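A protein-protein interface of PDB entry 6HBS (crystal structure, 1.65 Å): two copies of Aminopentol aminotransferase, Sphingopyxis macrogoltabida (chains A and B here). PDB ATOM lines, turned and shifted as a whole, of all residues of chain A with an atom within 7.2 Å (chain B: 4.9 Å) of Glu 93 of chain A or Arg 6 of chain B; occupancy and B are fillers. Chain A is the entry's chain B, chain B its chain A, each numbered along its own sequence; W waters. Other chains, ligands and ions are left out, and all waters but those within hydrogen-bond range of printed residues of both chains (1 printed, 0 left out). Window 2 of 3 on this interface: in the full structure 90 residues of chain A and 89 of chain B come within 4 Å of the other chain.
Of the printed residues of chain B, Leu 84 of chain A touches Arg 40. Of the printed residues of chain B, Pro 91 of chain A touches Phe 38 and Phe 39. Printed residues of chain B within 4 Å of Ser 92 of chain A: Phe 38 (3.6 Å) and Phe 39 (3.3 Å). Glu 93 of chain A touches just these residues of chain B: Arg 6, Leu 10, Phe 39, Arg 40 and Ala 50. Asn 97 of chain A touches none of the printed residues of chain B. Arg 6 of chain B touches one residue of chain A. Printed residues of chain A within 4 Å of Leu 10 of chain B: Glu 93 (3.4 Å) and Val 96 (3.9 Å). The nearest residue of chain B that does not touch Glu 93 of chain A is Phe 38 of chain B (4.1 Å). The nearest residue of chain A that does not touch Arg 6 of chain B is Asn 97 of chain A (7.0 Å).
Printed residues of chain A that touch a printed residue of chain B: Leu 84, Gly 90, Pro 91, Ser 92, Glu 93 and Val 96. Hydrophobic or aromatic side chains of chain A that line the printed part of chain B: Leu 84, Pro 91 and Val 96. Printed residues of chain B that touch a printed residue of chain A: Arg 6, Leu 10, Phe 38, Phe 39, Arg 40 and Ala 50. Hydrophobic or aromatic side chains of chain B that line the printed part of chain A: Leu 10, Phe 38, Phe 39 and Ala 50. Among the printed residues, 13 pairs touch across the chains. Among the printed residues, Asp or Glu carboxylates within 4 Å of a Lys or Arg side-chain nitrogen of the other chain: Glu 93 of chain A with Arg 6 of chain B.
No position is printed for both chains.
OE2 of Glu 93 of chain A is in salt-bridge range of NH1 of Arg 6 of chain B (2.6 Å). O of Phe 39 of chain B sits at hydrogen-bond distance from N of Glu 93 of chain A, at 3.0 Å. The backbone NH of Phe 39 of chain B sits at hydrogen-bond distance from the backbone carbonyl oxygen of Pro 91 of chain A, at 2.9 Å.
Water W1 lies within hydrogen-bond range of the side-chain hydroxyl of Ser 92 of chain A (2.7 Å), the backbone carbonyl oxygen of Arg 40 of chain B (2.8 Å) and the side-chain amide nitrogen of Gln 81 of chain A (2.9 Å).
Among the printed residues, merely in contact across the chains: Ser 92 of chain A with Phe 39 of chain B, Pro 91 of chain A with Phe 38 of chain B, Leu 84 of chain A with Arg 40 of chain B, Glu 93 of chain A with Leu 10 of chain B, Gly 90 of chain A with Phe 39 of chain B, Ser 92 of chain A with Phe 38 of chain B, Val 96 of chain A with Phe 38 of chain B, Glu 93 of chain A with Arg 40 of chain B, Glu 93 of chain A with Ala 50 of chain B and Val 96 of chain A with Leu 10 of chain B.
OG of Ser 92 of chain A is in hydrogen-bond range of N of Ile 94 of chain A (2.9 Å). OE1 of Gln 7 of chain B lies within hydrogen-bond range of N of Phe 38 of chain B (2.9 Å). The backbone carbonyl oxygen (O) of Phe 38 of chain B is in hydrogen-bond range of the backbone NH (N) of Ala 50 of chain B, at 3.1 Å. The backbone NH (N) of Arg 6 of chain B lies within hydrogen-bond range of the side-chain carboxylate (OD1) of Asp 51 of chain B (2.8 Å). NH1 of Arg 6 of chain B sits at hydrogen-bond distance from O of Ala 50 of chain B (2.6 Å).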
ATOM      1  N   GLN A  81     -23.013 -29.616   2.040  1.00  0.00           N
ATOM      2  CA  GLN A  81     -21.687 -29.703   2.638  1.00  0.00           C
ATOM      3  C   GLN A  81     -21.029 -31.035   2.267  1.00  0.00           C
ATOM      4  O   GLN A  81     -19.809 -31.130   2.079  1.00  0.00           O
ATOM      5  CB  GLN A  81     -21.764 -29.552   4.158  1.00  0.00           C
ATOM      6  CG  GLN A  81     -20.389 -29.563   4.816  1.00  0.00           C
ATOM      7  CD  GLN A  81     -19.521 -28.426   4.327  1.00  0.00           C
ATOM      8  OE1 GLN A  81     -20.021 -27.306   4.135  1.00  0.00           O
ATOM      9  NE2 GLN A  81     -18.212 -28.672   4.210  1.00  0.00           N
ATOM     10  N   LEU A  84     -18.815 -31.011  -0.551  1.00  0.00           N
ATOM     11  CA  LEU A  84     -17.572 -30.288  -0.316  1.00  0.00           C
ATOM     12  C   LEU A  84     -16.600 -31.169   0.486  1.00  0.00           C
ATOM     13  O   LEU A  84     -15.599 -31.648  -0.068  1.00  0.00           O
ATOM     14  CB  LEU A  84     -17.843 -28.953   0.379  1.00  0.00           C
ATOM     15  CG  LEU A  84     -18.690 -27.962  -0.422  1.00  0.00           C
ATOM     16  CD1 LEU A  84     -18.856 -26.677   0.349  1.00  0.00           C
ATOM     17  CD2 LEU A  84     -18.080 -27.680  -1.805  1.00  0.00           C
ATOM     18  N   MET A  88     -11.936 -33.808   7.518  1.00  0.00           N
ATOM     19  CA  MET A  88     -10.767 -33.406   6.721  1.00  0.00           C
ATOM     20  C   MET A  88      -9.584 -33.180   7.665  1.00  0.00           C
ATOM     21  O   MET A  88      -9.725 -33.267   8.871  1.00  0.00           O
ATOM     22  CB  MET A  88     -11.070 -32.127   5.930  1.00  0.00           C
ATOM     23  CG  MET A  88     -12.254 -32.280   4.978  1.00  0.00           C
ATOM     24  SD  MET A  88     -12.633 -30.802   4.013  1.00  0.00           S
ATOM     25  CE  MET A  88     -13.423 -29.710   5.195  1.00  0.00           C
ATOM     26  N   GLY A  90      -8.141 -30.468   8.394  1.00  0.00           N
ATOM     27  CA  GLY A  90      -8.542 -29.402   9.298  1.00  0.00           C
ATOM     28  C   GLY A  90     -10.038 -29.171   9.210  1.00  0.00           C
ATOM     29  O   GLY A  90     -10.712 -29.753   8.356  1.00  0.00           O
ATOM     30  N   PRO A  91     -10.606 -28.362  10.117  1.00  0.00           N
ATOM     31  CA  PRO A  91     -12.014 -28.021  10.034  1.00  0.00           C
ATOM     32  C   PRO A  91     -12.338 -27.262   8.735  1.00  0.00           C
ATOM     33  O   PRO A  91     -11.477 -26.541   8.212  1.00  0.00           O
ATOM     34  CB  PRO A  91     -12.220 -27.060  11.218  1.00  0.00           C
ATOM     35  CG  PRO A  91     -10.843 -26.523  11.487  1.00  0.00           C
ATOM     36  CD  PRO A  91      -9.926 -27.701  11.235  1.00  0.00           C
ATOM     37  N   SER A  92     -13.604 -27.339   8.326  1.00  0.00           N
ATOM     38  CA  SER A  92     -14.134 -26.490   7.311  1.00  0.00           C
ATOM     39  C   SER A  92     -14.192 -25.060   7.845  1.00  0.00           C
ATOM     40  O   SER A  92     -14.380 -24.830   9.060  1.00  0.00           O
ATOM     41  CB  SER A  92     -15.509 -26.940   6.830  1.00  0.00           C
ATOM     42  OG  SER A  92     -16.133 -25.899   6.075  1.00  0.00           O
ATOM     43  N   GLU A  93     -14.031 -24.106   6.922  1.00  0.00           N
ATOM     44  CA  GLU A  93     -14.361 -22.702   7.157  1.00  0.00           C
ATOM     45  C   GLU A  93     -15.737 -22.534   7.821  1.00  0.00           C
ATOM     46  O   GLU A  93     -15.927 -21.553   8.520  1.00  0.00           O
ATOM     47  CB  GLU A  93     -14.371 -21.901   5.851  1.00  0.00           C
ATOM     48  CG  GLU A  93     -15.290 -22.456   4.801  1.00  0.00           C
ATOM     49  CD  GLU A  93     -15.189 -21.748   3.451  1.00  0.00           C
ATOM     50  OE1 GLU A  93     -16.160 -21.781   2.717  1.00  0.00           O
ATOM     51  OE2 GLU A  93     -14.132 -21.191   3.149  1.00  0.00           O
ATOM     52  N   ILE A  94     -16.694 -23.442   7.594  1.00  0.00           N
ATOM     53  CA  ILE A  94     -18.034 -23.246   8.176  1.00  0.00           C
ATOM     54  C   ILE A  94     -18.012 -23.392   9.707  1.00  0.00           C
ATOM     55  O   ILE A  94     -19.003 -23.016  10.365  1.00  0.00           O
ATOM     56  CB  ILE A  94     -19.103 -24.145   7.535  1.00  0.00           C
ATOM     57  CG1 ILE A  94     -18.933 -25.610   7.922  1.00  0.00           C
ATOM     58  CG2 ILE A  94     -19.168 -23.939   6.012  1.00  0.00           C
ATOM     59  CD1 ILE A  94     -20.062 -26.476   7.493  1.00  0.00           C
ATOM     60  N   MET A  95     -16.922 -23.914  10.282  1.00  0.00           N
ATOM     61  CA  MET A  95     -16.806 -23.953  11.747  1.00  0.00           C
ATOM     62  C   MET A  95     -16.857 -22.537  12.318  1.00  0.00           C
ATOM     63  O   MET A  95     -17.463 -22.301  13.380  1.00  0.00           O
ATOM     64  CB  MET A  95     -15.523 -24.652  12.188  1.00  0.00           C
ATOM     65  CG  MET A  95     -15.373 -24.770  13.677  1.00  0.00           C
ATOM     66  SD  MET A  95     -13.811 -25.573  14.115  1.00  0.00           S
ATOM     67  CE  MET A  95     -14.033 -25.739  15.878  1.00  0.00           C
ATOM     68  N   VAL A  96     -16.287 -21.579  11.585  1.00  0.00           N
ATOM     69  CA  VAL A  96     -16.342 -20.200  12.006  1.00  0.00           C
ATOM     70  C   VAL A  96     -17.797 -19.674  11.985  1.00  0.00           C
ATOM     71  O   VAL A  96     -18.241 -19.079  12.983  1.00  0.00           O
ATOM     72  CB  VAL A  96     -15.357 -19.330  11.193  1.00  0.00           C
ATOM     73  CG1 VAL A  96     -15.362 -17.899  11.681  1.00  0.00           C
ATOM     74  CG2 VAL A  96     -13.942 -19.878  11.259  1.00  0.00           C
ATOM     75  N   ASN A  97     -18.524 -19.874  10.878  1.00  0.00           N
ATOM     76  CA  ASN A  97     -19.923 -19.492  10.749  1.00  0.00           C
ATOM     77  C   ASN A  97     -20.733 -20.098  11.919  1.00  0.00           C
ATOM     78  O   ASN A  97     -21.541 -19.391  12.544  1.00  0.00           O
ATOM     79  CB  ASN A  97     -20.509 -19.847   9.384  1.00  0.00           C
ATOM     80  CG  ASN A  97     -19.679 -19.387   8.185  1.00  0.00           C
ATOM     81  OD1 ASN A  97     -18.531 -18.930   8.289  1.00  0.00           O
ATOM     82  ND2 ASN A  97     -20.208 -19.610   7.006  1.00  0.00           N
ATOM     83  N   LEU A  98     -20.507 -21.378  12.228  1.00  0.00           N
ATOM     84  CA  LEU A  98     -21.252 -22.080  13.305  1.00  0.00           C
ATOM     85  C   LEU A  98     -21.000 -21.410  14.641  1.00  0.00           C
ATOM     86  O   LEU A  98     -21.969 -21.087  15.357  1.00  0.00           O
ATOM     87  CB  LEU A  98     -20.895 -23.563  13.402  1.00  0.00           C
ATOM     88  CG  LEU A  98     -21.586 -24.334  14.534  1.00  0.00           C
ATOM     89  CD1 LEU A  98     -23.110 -24.195  14.478  1.00  0.00           C
ATOM     90  CD2 LEU A  98     -21.182 -25.797  14.517  1.00  0.00           C
ATOM     91  N   ALA A 292     -17.276 -31.414   9.157  1.00  0.00           N
ATOM     92  CA  ALA A 292     -18.065 -30.303   8.612  1.00  0.00           C
ATOM     93  C   ALA A 292     -19.559 -30.630   8.476  1.00  0.00           C
ATOM     94  O   ALA A 292     -20.343 -29.749   8.601  1.00  0.00           O
ATOM     95  CB  ALA A 292     -17.502 -29.891   7.271  1.00  0.00           C
ATOM     96  N   MET A 295     -21.670 -29.841  11.334  1.00  0.00           N
ATOM     97  CA  MET A 295     -21.669 -28.397  11.500  1.00  0.00           C
ATOM     98  C   MET A 295     -22.614 -27.675  10.512  1.00  0.00           C
ATOM     99  O   MET A 295     -23.262 -26.660  10.889  1.00  0.00           O
ATOM    100  CB  MET A 295     -20.254 -27.832  11.368  1.00  0.00           C
ATOM    101  CG  MET A 295     -19.328 -28.320  12.485  1.00  0.00           C
ATOM    102  SD  MET A 295     -17.775 -27.442  12.436  1.00  0.00           S
ATOM    103  CE  MET A 295     -16.879 -28.377  13.673  1.00  0.00           C
ATOM    104  N   ILE A 299     -25.791 -25.403  11.577  1.00  0.00           N
ATOM    105  CA  ILE A 299     -26.033 -24.034  11.111  1.00  0.00           C
ATOM    106  C   ILE A 299     -27.497 -23.895  10.644  1.00  0.00           C
ATOM    107  O   ILE A 299     -28.151 -22.898  10.938  1.00  0.00           O
ATOM    108  CB  ILE A 299     -25.031 -23.627  10.009  1.00  0.00           C
ATOM    109  CG1 ILE A 299     -23.632 -23.399  10.579  1.00  0.00           C
ATOM    110  CG2 ILE A 299     -25.534 -22.414   9.242  1.00  0.00           C
ATOM    111  CD1 ILE A 299     -22.540 -23.361   9.525  1.00  0.00           C
ATOM    112  N   GLY B   4      -3.267 -15.657   1.384  1.00  0.00           N
ATOM    113  CA  GLY B   4      -4.493 -16.343   1.843  1.00  0.00           C
ATOM    114  C   GLY B   4      -5.497 -15.355   2.407  1.00  0.00           C
ATOM    115  O   GLY B   4      -5.630 -15.246   3.619  1.00  0.00           O
ATOM    116  N   THR B   5      -6.197 -14.641   1.516  1.00  0.00           N
ATOM    117  CA  THR B   5      -7.172 -13.608   1.886  1.00  0.00           C
ATOM    118  C   THR B   5      -8.298 -14.213   2.747  1.00  0.00           C
ATOM    119  O   THR B   5      -8.631 -13.667   3.829  1.00  0.00           O
ATOM    120  CB  THR B   5      -7.718 -12.898   0.639  1.00  0.00           C
ATOM    121  OG1 THR B   5      -6.674 -12.042   0.185  1.00  0.00           O
ATOM    122  CG2 THR B   5      -8.958 -12.067   0.886  1.00  0.00           C
ATOM    123  N   ARG B   6      -8.888 -15.309   2.257  1.00  0.00           N
ATOM    124  CA  ARG B   6      -9.997 -15.983   2.933  1.00  0.00           C
ATOM    125  C   ARG B   6      -9.473 -16.571   4.245  1.00  0.00           C
ATOM    126  O   ARG B   6     -10.120 -16.432   5.263  1.00  0.00           O
ATOM    127  CB  ARG B   6     -10.684 -17.016   2.035  1.00  0.00           C
ATOM    128  CG  ARG B   6     -11.419 -16.379   0.860  1.00  0.00           C
ATOM    129  CD  ARG B   6     -12.352 -17.322   0.109  1.00  0.00           C
ATOM    130  NE  ARG B   6     -13.561 -17.568   0.889  1.00  0.00           N
ATOM    131  CZ  ARG B   6     -13.967 -18.754   1.378  1.00  0.00           C
ATOM    132  NH1 ARG B   6     -13.376 -19.900   1.044  1.00  0.00           N
ATOM    133  NH2 ARG B   6     -15.013 -18.776   2.189  1.00  0.00           N
ATOM    134  N   GLN B   7      -8.277 -17.159   4.223  1.00  0.00           N
ATOM    135  CA  GLN B   7      -7.714 -17.783   5.434  1.00  0.00           C
ATOM    136  C   GLN B   7      -7.522 -16.733   6.538  1.00  0.00           C
ATOM    137  O   GLN B   7      -7.806 -16.990   7.724  1.00  0.00           O
ATOM    138  CB  GLN B   7      -6.389 -18.482   5.117  1.00  0.00           C
ATOM    139  CG  GLN B   7      -5.898 -19.442   6.186  1.00  0.00           C
ATOM    140  CD  GLN B   7      -6.747 -20.677   6.396  1.00  0.00           C
ATOM    141  OE1 GLN B   7      -6.970 -21.093   7.542  1.00  0.00           O
ATOM    142  NE2 GLN B   7      -7.211 -21.282   5.304  1.00  0.00           N
ATOM    143  N   LYS B   8      -7.017 -15.562   6.144  1.00  0.00           N
ATOM    144  CA  LYS B   8      -6.728 -14.519   7.067  1.00  0.00           C
ATOM    145  C   LYS B   8      -8.031 -14.021   7.722  1.00  0.00           C
ATOM    146  O   LYS B   8      -8.029 -13.738   8.945  1.00  0.00           O
ATOM    147  CB  LYS B   8      -5.992 -13.373   6.370  1.00  0.00           C
ATOM    148  CG  LYS B   8      -5.739 -12.186   7.284  1.00  0.00           C
ATOM    149  CD  LYS B   8      -5.114 -10.991   6.617  1.00  0.00           C
ATOM    150  CE  LYS B   8      -4.653  -9.962   7.628  1.00  0.00           C
ATOM    151  NZ  LYS B   8      -4.579  -8.617   7.018  1.00  0.00           N
ATOM    152  N   ASP B   9      -9.077 -13.831   6.900  1.00  0.00           N
ATOM    153  CA  ASP B   9     -10.419 -13.385   7.348  1.00  0.00           C
ATOM    154  C   ASP B   9     -10.948 -14.394   8.385  1.00  0.00           C
ATOM    155  O   ASP B   9     -11.447 -13.995   9.459  1.00  0.00           O
ATOM    156  CB  ASP B   9     -11.411 -13.260   6.182  1.00  0.00           C
ATOM    157  CG  ASP B   9     -12.837 -12.865   6.568  1.00  0.00           C
ATOM    158  OD1 ASP B   9     -12.999 -11.797   7.181  1.00  0.00           O
ATOM    159  OD2 ASP B   9     -13.770 -13.684   6.322  1.00  0.00           O
ATOM    160  N   LEU B  10     -10.843 -15.684   8.031  1.00  0.00           N
ATOM    161  CA  LEU B  10     -11.373 -16.784   8.813  1.00  0.00           C
ATOM    162  C   LEU B  10     -10.620 -16.875  10.146  1.00  0.00           C
ATOM    163  O   LEU B  10     -11.243 -17.055  11.166  1.00  0.00           O
ATOM    164  CB  LEU B  10     -11.266 -18.081   8.008  1.00  0.00           C
ATOM    165  CG  LEU B  10     -12.365 -18.286   6.968  1.00  0.00           C
ATOM    166  CD1 LEU B  10     -12.020 -19.434   6.037  1.00  0.00           C
ATOM    167  CD2 LEU B  10     -13.713 -18.539   7.643  1.00  0.00           C
ATOM    168  N   PHE B  38      -8.163 -23.683   8.055  1.00  0.00           N
ATOM    169  CA  PHE B  38      -9.508 -23.905   7.582  1.00  0.00           C
ATOM    170  C   PHE B  38      -9.529 -24.348   6.116  1.00  0.00           C
ATOM    171  O   PHE B  38      -8.866 -23.743   5.302  1.00  0.00           O
ATOM    172  CB  PHE B  38     -10.316 -22.621   7.769  1.00  0.00           C
ATOM    173  CG  PHE B  38     -10.525 -22.285   9.216  1.00  0.00           C
ATOM    174  CD1 PHE B  38     -11.385 -23.057   9.982  1.00  0.00           C
ATOM    175  CD2 PHE B  38      -9.803 -21.274   9.820  1.00  0.00           C
ATOM    176  CE1 PHE B  38     -11.572 -22.778  11.320  1.00  0.00           C
ATOM    177  CE2 PHE B  38      -9.975 -21.000  11.165  1.00  0.00           C
ATOM    178  CZ  PHE B  38     -10.871 -21.748  11.909  1.00  0.00           C
ATOM    179  N   PHE B  39     -10.354 -25.345   5.802  1.00  0.00           N
ATOM    180  CA  PHE B  39     -10.451 -25.954   4.473  1.00  0.00           C
ATOM    181  C   PHE B  39     -11.845 -25.764   3.860  1.00  0.00           C
ATOM    182  O   PHE B  39     -12.798 -25.370   4.552  1.00  0.00           O
ATOM    183  CB  PHE B  39     -10.070 -27.426   4.550  1.00  0.00           C
ATOM    184  CG  PHE B  39      -8.646 -27.604   4.982  1.00  0.00           C
ATOM    185  CD1 PHE B  39      -8.296 -27.530   6.326  1.00  0.00           C
ATOM    186  CD2 PHE B  39      -7.640 -27.780   4.038  1.00  0.00           C
ATOM    187  CE1 PHE B  39      -6.967 -27.655   6.706  1.00  0.00           C
ATOM    188  CE2 PHE B  39      -6.313 -27.896   4.424  1.00  0.00           C
ATOM    189  CZ  PHE B  39      -5.982 -27.849   5.755  1.00  0.00           C
ATOM    190  N   ARG B  40     -11.948 -25.986   2.543  1.00  0.00           N
ATOM    191  CA  ARG B  40     -13.221 -25.795   1.835  1.00  0.00           C
ATOM    192  C   ARG B  40     -13.775 -27.131   1.342  1.00  0.00           C
ATOM    193  O   ARG B  40     -14.999 -27.364   1.355  1.00  0.00           O
ATOM    194  CB  ARG B  40     -13.092 -24.756   0.715  1.00  0.00           C
ATOM    195  CG  ARG B  40     -14.444 -24.168   0.319  1.00  0.00           C
ATOM    196  CD  ARG B  40     -14.404 -23.193  -0.843  1.00  0.00           C
ATOM    197  NE  ARG B  40     -14.279 -23.921  -2.100  1.00  0.00           N
ATOM    198  CZ  ARG B  40     -15.288 -24.467  -2.774  1.00  0.00           C
ATOM    199  NH1 ARG B  40     -16.526 -24.367  -2.307  1.00  0.00           N
ATOM    200  NH2 ARG B  40     -15.057 -25.100  -3.911  1.00  0.00           N
ATOM    201  N   ALA B  50      -9.197 -22.807   2.363  1.00  0.00           N
ATOM    202  CA  ALA B  50     -10.267 -21.799   2.171  1.00  0.00           C
ATOM    203  C   ALA B  50     -10.017 -20.967   0.895  1.00  0.00           C
ATOM    204  O   ALA B  50     -10.957 -20.439   0.343  1.00  0.00           O
ATOM    205  CB  ALA B  50     -10.345 -20.890   3.364  1.00  0.00           C
ATOM    206  N   ASP B  51      -8.747 -20.813   0.494  1.00  0.00           N
ATOM    207  CA  ASP B  51      -8.341 -19.987  -0.672  1.00  0.00           C
ATOM    208  C   ASP B  51      -8.180 -20.841  -1.929  1.00  0.00           C
ATOM    209  O   ASP B  51      -7.594 -20.380  -2.902  1.00  0.00           O
ATOM    210  CB  ASP B  51      -7.078 -19.181  -0.346  1.00  0.00           C
ATOM    211  CG  ASP B  51      -7.349 -18.048   0.625  1.00  0.00           C
ATOM    212  OD1 ASP B  51      -7.965 -17.051   0.206  1.00  0.00           O
ATOM    213  OD2 ASP B  51      -6.983 -18.179   1.821  1.00  0.00           O
HETATM  214  O   HOH W   1     -16.607 -26.430   3.438  1.00  0.00           O
